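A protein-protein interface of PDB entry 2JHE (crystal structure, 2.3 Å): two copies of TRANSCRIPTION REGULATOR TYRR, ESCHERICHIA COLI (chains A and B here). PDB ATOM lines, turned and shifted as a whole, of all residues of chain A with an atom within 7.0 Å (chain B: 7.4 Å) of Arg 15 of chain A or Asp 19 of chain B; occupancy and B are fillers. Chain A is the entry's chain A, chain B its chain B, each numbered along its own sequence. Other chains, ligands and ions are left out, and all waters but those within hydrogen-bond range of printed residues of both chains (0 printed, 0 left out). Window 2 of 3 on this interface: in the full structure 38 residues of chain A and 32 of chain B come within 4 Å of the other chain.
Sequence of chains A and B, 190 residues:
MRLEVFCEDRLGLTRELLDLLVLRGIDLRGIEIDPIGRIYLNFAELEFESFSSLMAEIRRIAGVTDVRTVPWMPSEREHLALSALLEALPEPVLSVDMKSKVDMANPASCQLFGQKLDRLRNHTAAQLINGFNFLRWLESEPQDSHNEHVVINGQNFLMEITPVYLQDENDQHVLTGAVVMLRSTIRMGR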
ATOM      1  N   GLY A  12     -16.273 -11.947  -7.824  1.00  0.00           N
ATOM      2  CA  GLY A  12     -16.150 -11.867  -9.295  1.00  0.00           C
ATOM      3  C   GLY A  12     -14.883 -11.199  -9.818  1.00  0.00           C
ATOM      4  O   GLY A  12     -14.711 -11.043 -11.035  1.00  0.00           O
ATOM      5  N   LEU A  13     -13.967 -10.836  -8.924  1.00  0.00           N
ATOM      6  CA  LEU A  13     -12.798 -10.033  -9.345  1.00  0.00           C
ATOM      7  C   LEU A  13     -11.794 -10.889 -10.164  1.00  0.00           C
ATOM      8  O   LEU A  13     -11.231 -10.451 -11.191  1.00  0.00           O
ATOM      9  CB  LEU A  13     -12.144  -9.409  -8.120  1.00  0.00           C
ATOM     10  CG  LEU A  13     -11.207  -8.224  -8.293  1.00  0.00           C
ATOM     11  CD1 LEU A  13     -11.146  -7.538  -6.974  1.00  0.00           C
ATOM     12  CD2 LEU A  13      -9.856  -8.751  -8.736  1.00  0.00           C
ATOM     13  N   THR A  14     -11.620 -12.121  -9.732  1.00  0.00           N
ATOM     14  CA  THR A  14     -10.700 -13.027 -10.370  1.00  0.00           C
ATOM     15  C   THR A  14     -11.133 -13.399 -11.794  1.00  0.00           C
ATOM     16  O   THR A  14     -10.281 -13.517 -12.673  1.00  0.00           O
ATOM     17  CB  THR A  14     -10.522 -14.308  -9.508  1.00  0.00           C
ATOM     18  OG1 THR A  14      -9.861 -13.980  -8.266  1.00  0.00           O
ATOM     19  CG2 THR A  14      -9.610 -15.270 -10.235  1.00  0.00           C
ATOM     20  N   ARG A  15     -12.436 -13.638 -11.983  1.00  0.00           N
ATOM     21  CA  ARG A  15     -13.088 -13.856 -13.278  1.00  0.00           C
ATOM     22  C   ARG A  15     -12.939 -12.648 -14.239  1.00  0.00           C
ATOM     23  O   ARG A  15     -12.674 -12.802 -15.423  1.00  0.00           O
ATOM     24  CB  ARG A  15     -14.584 -14.118 -13.053  1.00  0.00           C
ATOM     25  CG  ARG A  15     -15.409 -14.278 -14.322  1.00  0.00           C
ATOM     26  CD  ARG A  15     -15.372 -15.722 -14.949  1.00  0.00           C
ATOM     27  NE  ARG A  15     -15.586 -15.617 -16.391  1.00  0.00           N
ATOM     28  CZ  ARG A  15     -16.701 -15.911 -17.055  1.00  0.00           C
ATOM     29  NH1 ARG A  15     -17.772 -16.437 -16.445  1.00  0.00           N
ATOM     30  NH2 ARG A  15     -16.728 -15.698 -18.362  1.00  0.00           N
ATOM     31  N   GLU A  16     -13.160 -11.454 -13.712  1.00  0.00           N
ATOM     32  CA  GLU A  16     -13.160 -10.278 -14.507  1.00  0.00           C
ATOM     33  C   GLU A  16     -11.725 -10.061 -15.004  1.00  0.00           C
ATOM     34  O   GLU A  16     -11.537  -9.647 -16.137  1.00  0.00           O
ATOM     35  CB  GLU A  16     -13.708  -9.114 -13.681  1.00  0.00           C
ATOM     36  CG  GLU A  16     -14.632  -8.192 -14.399  1.00  0.00           C
ATOM     37  CD  GLU A  16     -14.832  -6.885 -13.656  1.00  0.00           C
ATOM     38  OE1 GLU A  16     -15.290  -6.942 -12.487  1.00  0.00           O
ATOM     39  OE2 GLU A  16     -14.509  -5.810 -14.238  1.00  0.00           O
ATOM     40  N   LEU A  17     -10.728 -10.436 -14.190  1.00  0.00           N
ATOM     41  CA  LEU A  17      -9.287 -10.417 -14.581  1.00  0.00           C
ATOM     42  C   LEU A  17      -8.956 -11.435 -15.654  1.00  0.00           C
ATOM     43  O   LEU A  17      -8.252 -11.100 -16.592  1.00  0.00           O
ATOM     44  CB  LEU A  17      -8.366 -10.720 -13.402  1.00  0.00           C
ATOM     45  CG  LEU A  17      -7.937  -9.681 -12.398  1.00  0.00           C
ATOM     46  CD1 LEU A  17      -7.098 -10.425 -11.384  1.00  0.00           C
ATOM     47  CD2 LEU A  17      -7.209  -8.421 -13.011  1.00  0.00           C
ATOM     48  N   LEU A  18      -9.416 -12.687 -15.487  1.00  0.00           N
ATOM     49  CA  LEU A  18      -9.216 -13.657 -16.546  1.00  0.00           C
ATOM     50  C   LEU A  18      -9.946 -13.283 -17.813  1.00  0.00           C
ATOM     51  O   LEU A  18      -9.413 -13.511 -18.885  1.00  0.00           O
ATOM     52  CB  LEU A  18      -9.594 -15.096 -16.157  1.00  0.00           C
ATOM     53  CG  LEU A  18      -8.780 -15.764 -15.019  1.00  0.00           C
ATOM     54  CD1 LEU A  18      -9.017 -17.272 -15.032  1.00  0.00           C
ATOM     55  CD2 LEU A  18      -7.326 -15.413 -15.030  1.00  0.00           C
ATOM     56  N   ASP A  19     -11.171 -12.751 -17.715  1.00  0.00           N
ATOM     57  CA  ASP A  19     -11.861 -12.262 -18.932  1.00  0.00           C
ATOM     58  C   ASP A  19     -10.976 -11.232 -19.648  1.00  0.00           C
ATOM     59  O   ASP A  19     -10.839 -11.233 -20.848  1.00  0.00           O
ATOM     60  CB  ASP A  19     -13.175 -11.548 -18.585  1.00  0.00           C
ATOM     61  CG  ASP A  19     -14.290 -12.501 -18.112  1.00  0.00           C
ATOM     62  OD1 ASP A  19     -14.300 -13.690 -18.453  1.00  0.00           O
ATOM     63  OD2 ASP A  19     -15.173 -12.004 -17.382  1.00  0.00           O
ATOM     64  N   LEU A  20     -10.400 -10.334 -18.862  1.00  0.00           N
ATOM     65  CA  LEU A  20      -9.601  -9.253 -19.411  1.00  0.00           C
ATOM     66  C   LEU A  20      -8.351  -9.771 -20.155  1.00  0.00           C
ATOM     67  O   LEU A  20      -8.058  -9.301 -21.226  1.00  0.00           O
ATOM     68  CB  LEU A  20      -9.239  -8.272 -18.318  1.00  0.00           C
ATOM     69  CG  LEU A  20      -8.335  -7.149 -18.853  1.00  0.00           C
ATOM     70  CD1 LEU A  20      -8.992  -6.440 -20.061  1.00  0.00           C
ATOM     71  CD2 LEU A  20      -8.022  -6.211 -17.755  1.00  0.00           C
ATOM     72  N   LEU A  21      -7.622 -10.716 -19.566  1.00  0.00           N
ATOM     73  CA  LEU A  21      -6.552 -11.433 -20.269  1.00  0.00           C
ATOM     74  C   LEU A  21      -7.033 -12.081 -21.540  1.00  0.00           C
ATOM     75  O   LEU A  21      -6.381 -11.958 -22.582  1.00  0.00           O
ATOM     76  CB  LEU A  21      -5.917 -12.495 -19.360  1.00  0.00           C
ATOM     77  CG  LEU A  21      -5.237 -11.973 -18.071  1.00  0.00           C
ATOM     78  CD1 LEU A  21      -4.622 -13.140 -17.377  1.00  0.00           C
ATOM     79  CD2 LEU A  21      -4.172 -10.857 -18.331  1.00  0.00           C
ATOM     80  N   ILE A  31      -2.490 -18.637 -12.286  1.00  0.00           N
ATOM     81  CA  ILE A  31      -3.014 -17.611 -11.407  1.00  0.00           C
ATOM     82  C   ILE A  31      -2.921 -18.179 -10.009  1.00  0.00           C
ATOM     83  O   ILE A  31      -3.271 -19.322  -9.791  1.00  0.00           O
ATOM     84  CB  ILE A  31      -4.464 -17.128 -11.806  1.00  0.00           C
ATOM     85  CG1 ILE A  31      -5.116 -16.395 -10.661  1.00  0.00           C
ATOM     86  CG2 ILE A  31      -5.355 -18.276 -12.175  1.00  0.00           C
ATOM     87  CD1 ILE A  31      -6.304 -15.510 -11.054  1.00  0.00           C
ATOM     88  N   ILE A  39      -3.444 -11.259  -5.905  1.00  0.00           N
ATOM     89  CA  ILE A  39      -3.614 -12.180  -7.007  1.00  0.00           C
ATOM     90  C   ILE A  39      -2.326 -12.092  -7.910  1.00  0.00           C
ATOM     91  O   ILE A  39      -1.960 -10.997  -8.377  1.00  0.00           O
ATOM     92  CB  ILE A  39      -4.913 -11.821  -7.826  1.00  0.00           C
ATOM     93  CG1 ILE A  39      -6.151 -11.942  -6.955  1.00  0.00           C
ATOM     94  CG2 ILE A  39      -5.068 -12.711  -9.053  1.00  0.00           C
ATOM     95  CD1 ILE A  39      -7.491 -11.727  -7.718  1.00  0.00           C
ATOM     96  N   GLY B  12     -13.546 -20.783 -22.685  1.00  0.00           N
ATOM     97  CA  GLY B  12     -14.271 -20.491 -21.448  1.00  0.00           C
ATOM     98  C   GLY B  12     -14.188 -21.515 -20.334  1.00  0.00           C
ATOM     99  O   GLY B  12     -14.680 -21.271 -19.237  1.00  0.00           O
ATOM    100  N   LEU B  13     -13.573 -22.658 -20.610  1.00  0.00           N
ATOM    101  CA  LEU B  13     -13.506 -23.739 -19.656  1.00  0.00           C
ATOM    102  C   LEU B  13     -12.777 -23.359 -18.354  1.00  0.00           C
ATOM    103  O   LEU B  13     -13.304 -23.597 -17.255  1.00  0.00           O
ATOM    104  CB  LEU B  13     -12.818 -24.950 -20.295  1.00  0.00           C
ATOM    105  CG  LEU B  13     -13.126 -26.295 -19.641  1.00  0.00           C
ATOM    106  CD1 LEU B  13     -13.208 -27.325 -20.746  1.00  0.00           C
ATOM    107  CD2 LEU B  13     -12.068 -26.673 -18.575  1.00  0.00           C
ATOM    108  N   THR B  14     -11.583 -22.778 -18.485  1.00  0.00           N
ATOM    109  CA  THR B  14     -10.734 -22.442 -17.339  1.00  0.00           C
ATOM    110  C   THR B  14     -11.519 -21.569 -16.377  1.00  0.00           C
ATOM    111  O   THR B  14     -11.528 -21.834 -15.175  1.00  0.00           O
ATOM    112  CB  THR B  14      -9.432 -21.707 -17.776  1.00  0.00           C
ATOM    113  OG1 THR B  14      -8.614 -22.605 -18.543  1.00  0.00           O
ATOM    114  CG2 THR B  14      -8.593 -21.269 -16.565  1.00  0.00           C
ATOM    115  N   ARG B  15     -12.205 -20.571 -16.935  1.00  0.00           N
ATOM    116  CA  ARG B  15     -12.970 -19.593 -16.181  1.00  0.00           C
ATOM    117  C   ARG B  15     -14.243 -20.148 -15.600  1.00  0.00           C
ATOM    118  O   ARG B  15     -14.717 -19.658 -14.588  1.00  0.00           O
ATOM    119  CB  ARG B  15     -13.283 -18.373 -17.043  1.00  0.00           C
ATOM    120  CG  ARG B  15     -12.073 -17.458 -17.262  1.00  0.00           C
ATOM    121  CD  ARG B  15     -12.376 -16.390 -18.393  1.00  0.00           C
ATOM    122  NE  ARG B  15     -12.527 -17.035 -19.681  1.00  0.00           N
ATOM    123  CZ  ARG B  15     -13.030 -16.461 -20.764  1.00  0.00           C
ATOM    124  NH1 ARG B  15     -13.483 -15.200 -20.707  1.00  0.00           N
ATOM    125  NH2 ARG B  15     -13.103 -17.161 -21.894  1.00  0.00           N
ATOM    126  N   GLU B  16     -14.790 -21.180 -16.241  1.00  0.00           N
ATOM    127  CA  GLU B  16     -15.992 -21.806 -15.772  1.00  0.00           C
ATOM    128  C   GLU B  16     -15.602 -22.699 -14.596  1.00  0.00           C
ATOM    129  O   GLU B  16     -16.305 -22.809 -13.588  1.00  0.00           O
ATOM    130  CB  GLU B  16     -16.690 -22.564 -16.948  1.00  0.00           C
ATOM    131  CG  GLU B  16     -17.734 -23.581 -16.503  1.00  0.00           C
ATOM    132  CD  GLU B  16     -18.504 -24.183 -17.660  1.00  0.00           C
ATOM    133  OE1 GLU B  16     -18.262 -23.773 -18.824  1.00  0.00           O
ATOM    134  OE2 GLU B  16     -19.350 -25.067 -17.397  1.00  0.00           O
ATOM    135  N   LEU B  17     -14.445 -23.313 -14.716  1.00  0.00           N
ATOM    136  CA  LEU B  17     -13.821 -24.040 -13.627  1.00  0.00           C
ATOM    137  C   LEU B  17     -13.524 -23.164 -12.395  1.00  0.00           C
ATOM    138  O   LEU B  17     -13.745 -23.596 -11.263  1.00  0.00           O
ATOM    139  CB  LEU B  17     -12.511 -24.545 -14.161  1.00  0.00           C
ATOM    140  CG  LEU B  17     -12.044 -25.960 -14.101  1.00  0.00           C
ATOM    141  CD1 LEU B  17     -10.518 -25.976 -14.410  1.00  0.00           C
ATOM    142  CD2 LEU B  17     -12.378 -26.526 -12.708  1.00  0.00           C
ATOM    143  N   LEU B  18     -13.005 -21.951 -12.613  1.00  0.00           N
ATOM    144  CA  LEU B  18     -12.769 -20.937 -11.557  1.00  0.00           C
ATOM    145  C   LEU B  18     -14.097 -20.460 -10.884  1.00  0.00           C
ATOM    146  O   LEU B  18     -14.175 -20.328  -9.656  1.00  0.00           O
ATOM    147  CB  LEU B  18     -12.001 -19.713 -12.147  1.00  0.00           C
ATOM    148  CG  LEU B  18     -11.894 -18.394 -11.333  1.00  0.00           C
ATOM    149  CD1 LEU B  18     -10.863 -18.503 -10.225  1.00  0.00           C
ATOM    150  CD2 LEU B  18     -11.571 -17.199 -12.205  1.00  0.00           C
ATOM    151  N   ASP B  19     -15.116 -20.213 -11.706  1.00  0.00           N
ATOM    152  CA  ASP B  19     -16.465 -19.881 -11.237  1.00  0.00           C
ATOM    153  C   ASP B  19     -16.975 -21.032 -10.366  1.00  0.00           C
ATOM    154  O   ASP B  19     -17.550 -20.795  -9.346  1.00  0.00           O
ATOM    155  CB  ASP B  19     -17.459 -19.674 -12.406  1.00  0.00           C
ATOM    156  CG  ASP B  19     -17.189 -18.401 -13.225  1.00  0.00           C
ATOM    157  OD1 ASP B  19     -16.241 -17.650 -12.887  1.00  0.00           O
ATOM    158  OD2 ASP B  19     -17.966 -18.155 -14.215  1.00  0.00           O
ATOM    159  N   LEU B  20     -16.740 -22.271 -10.760  1.00  0.00           N
ATOM    160  CA  LEU B  20     -17.258 -23.390  -9.962  1.00  0.00           C
ATOM    161  C   LEU B  20     -16.697 -23.341  -8.545  1.00  0.00           C
ATOM    162  O   LEU B  20     -17.427 -23.531  -7.590  1.00  0.00           O
ATOM    163  CB  LEU B  20     -16.957 -24.743 -10.616  1.00  0.00           C
ATOM    164  CG  LEU B  20     -17.382 -26.058  -9.920  1.00  0.00           C
ATOM    165  CD1 LEU B  20     -18.888 -26.074  -9.657  1.00  0.00           C
ATOM    166  CD2 LEU B  20     -17.019 -27.262 -10.804  1.00  0.00           C
ATOM    167  N   LEU B  21     -15.387 -23.156  -8.431  1.00  0.00           N
ATOM    168  CA  LEU B  21     -14.698 -23.156  -7.149  1.00  0.00           C
ATOM    169  C   LEU B  21     -15.020 -21.918  -6.318  1.00  0.00           C
ATOM    170  O   LEU B  21     -15.276 -22.033  -5.110  1.00  0.00           O
ATOM    171  CB  LEU B  21     -13.173 -23.380  -7.339  1.00  0.00           C
ATOM    172  CG  LEU B  21     -12.775 -24.880  -7.463  1.00  0.00           C
ATOM    173  CD1 LEU B  21     -12.791 -25.312  -8.904  1.00  0.00           C
ATOM    174  CD2 LEU B  21     -11.371 -25.113  -6.953  1.00  0.00           C
ATOM    175  N   VAL B  22     -15.069 -20.744  -6.963  1.00  0.00           N
ATOM    176  CA  VAL B  22     -15.574 -19.557  -6.282  1.00  0.00           C
ATOM    177  C   VAL B  22     -16.927 -19.825  -5.647  1.00  0.00           C
ATOM    178  O   VAL B  22     -17.118 -19.595  -4.461  1.00  0.00           O
ATOM    179  CB  VAL B  22     -15.612 -18.330  -7.221  1.00  0.00           C
ATOM    180  CG1 VAL B  22     -16.438 -17.165  -6.621  1.00  0.00           C
ATOM    181  CG2 VAL B  22     -14.215 -17.850  -7.492  1.00  0.00           C
ATOM    182  N   LEU B  23     -17.864 -20.333  -6.445  1.00  0.00           N
ATOM    183  CA  LEU B  23     -19.226 -20.603  -6.017  1.00  0.00           C
ATOM    184  C   LEU B  23     -19.372 -21.674  -4.926  1.00  0.00           C
ATOM    185  O   LEU B  23     -20.245 -21.541  -4.071  1.00  0.00           O
ATOM    186  CB  LEU B  23     -20.112 -20.954  -7.224  1.00  0.00           C
ATOM    187  CG  LEU B  23     -20.273 -19.808  -8.238  1.00  0.00           C
ATOM    188  CD1 LEU B  23     -20.815 -20.373  -9.561  1.00  0.00           C
ATOM    189  CD2 LEU B  23     -21.132 -18.637  -7.749  1.00  0.00           C
ATOM    190  N   ARG B  24     -18.545 -22.729  -4.980  1.00  0.00           N
ATOM    191  CA  ARG B  24     -18.576 -23.738  -3.924  1.00  0.00           C
ATOM    192  C   ARG B  24     -17.800 -23.241  -2.722  1.00  0.00           C
ATOM    193  O   ARG B  24     -17.553 -23.998  -1.820  1.00  0.00           O
ATOM    194  CB  ARG B  24     -18.058 -25.142  -4.363  1.00  0.00           C
ATOM    195  CG  ARG B  24     -18.694 -25.798  -5.606  1.00  0.00           C
ATOM    196  CD  ARG B  24     -20.190 -26.125  -5.431  1.00  0.00           C
ATOM    197  NE  ARG B  24     -20.990 -25.533  -6.523  1.00  0.00           N
ATOM    198  CZ  ARG B  24     -22.326 -25.475  -6.596  1.00  0.00           C
ATOM    199  NH1 ARG B  24     -23.116 -25.989  -5.645  1.00  0.00           N
ATOM    200  NH2 ARG B  24     -22.873 -24.884  -7.654  1.00  0.00           N
ATOM    201  N   GLY B  25     -17.417 -21.969  -2.700  1.00  0.00           N
ATOM    202  CA  GLY B  25     -16.598 -21.440  -1.603  1.00  0.00           C
ATOM    203  C   GLY B  25     -15.233 -22.114  -1.371  1.00  0.00           C
ATOM    204  O   GLY B  25     -14.723 -22.126  -0.265  1.00  0.00           O
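Of the 12 printed residues of chain A, 4 touch a printed residue of chain B. Hydrophobic or aromatic side chains of chain A within 4 Å of the printed part of chain B: Leu 18. Of the 14 printed residues of chain B, 3 touch a printed residue of chain A. Hydrophobic or aromatic side chains of chain B that line the printed part of chain A: Leu 18. Along chain B the printed residues that touch a printed residue of chain A span positions 15 to 19.
The side-chain carboxylate of Asp 19 of chain B lies within salt-bridge range of the guanidinium group of Arg 15 of chain A, at 2.8 Å. The side-chain carboxylate of Asp 19 of chain A lies within salt-bridge range of the guanidinium group of Arg 15 of chain B (2.8 Å).
Of chain B, only Arg 15 (3.7 Å), Leu 18 (3.7 Å) and Asp 19 (2.8 Å) come within 4 Å of Arg 15 of chain A. Printed residues of chain B within 4 Å of Leu 18 of chain A: Arg 15 (3.6 Å) and Leu 18 (3.8 Å). Leu 20 of chain A touches none of the printed residues of chain B. Printed residues of chain A within 4 Å of Arg 15 of chain B: Arg 15, Leu 18 and Asp 19. Of the printed residues of chain A, Leu 18 of chain B touches Thr 14, Arg 15 and Leu 18. Leu 21 of chain B touches none of the printed residues of chain A. The nearest residue of chain B that does not touch Arg 15 of chain A is Glu 16 of chain B (5.6 Å).
The side-chain carboxylate of Asp 19 of chain A is in salt-bridge range of the guanidinium group of Arg 15 of chain A (3.1 Å).
Thr 14 of chain A touches Leu 18 of chain B. Arg 15 of chain B touches Arg 15 of chain A. Leu 18 of chain B touches Arg 15 of chain A. CG of Arg 15 of chain B touches CB of Leu 18 of chain A (3.6 Å). Leu 18 of chain A touches Leu 18 of chain B.
Thr 14 of chain A touches Leu 18 of chain B, but with the chains exchanged Leu 18 of chain A does not touch Thr 14 of chain B (4.3 Å). Arg 15 of chain B touches its own counterpart, Arg 15 of chain A. Arg 15 of chain A touches Leu 18 of chain B, and with the chains exchanged Leu 18 of chain A touches Arg 15 of chain B. Arg 15 of chain A touches Asp 19 of chain B, and with the chains exchanged Asp 19 of chain A touches Arg 15 of chain B. Positions printed for both chains: 12, 13, 14, 15, 16, 17, 18, 19, 20 and 21. Of the 7 pairs that touch across the chains among the printed residues, 6 have their exchanged pair printed and touching as well.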
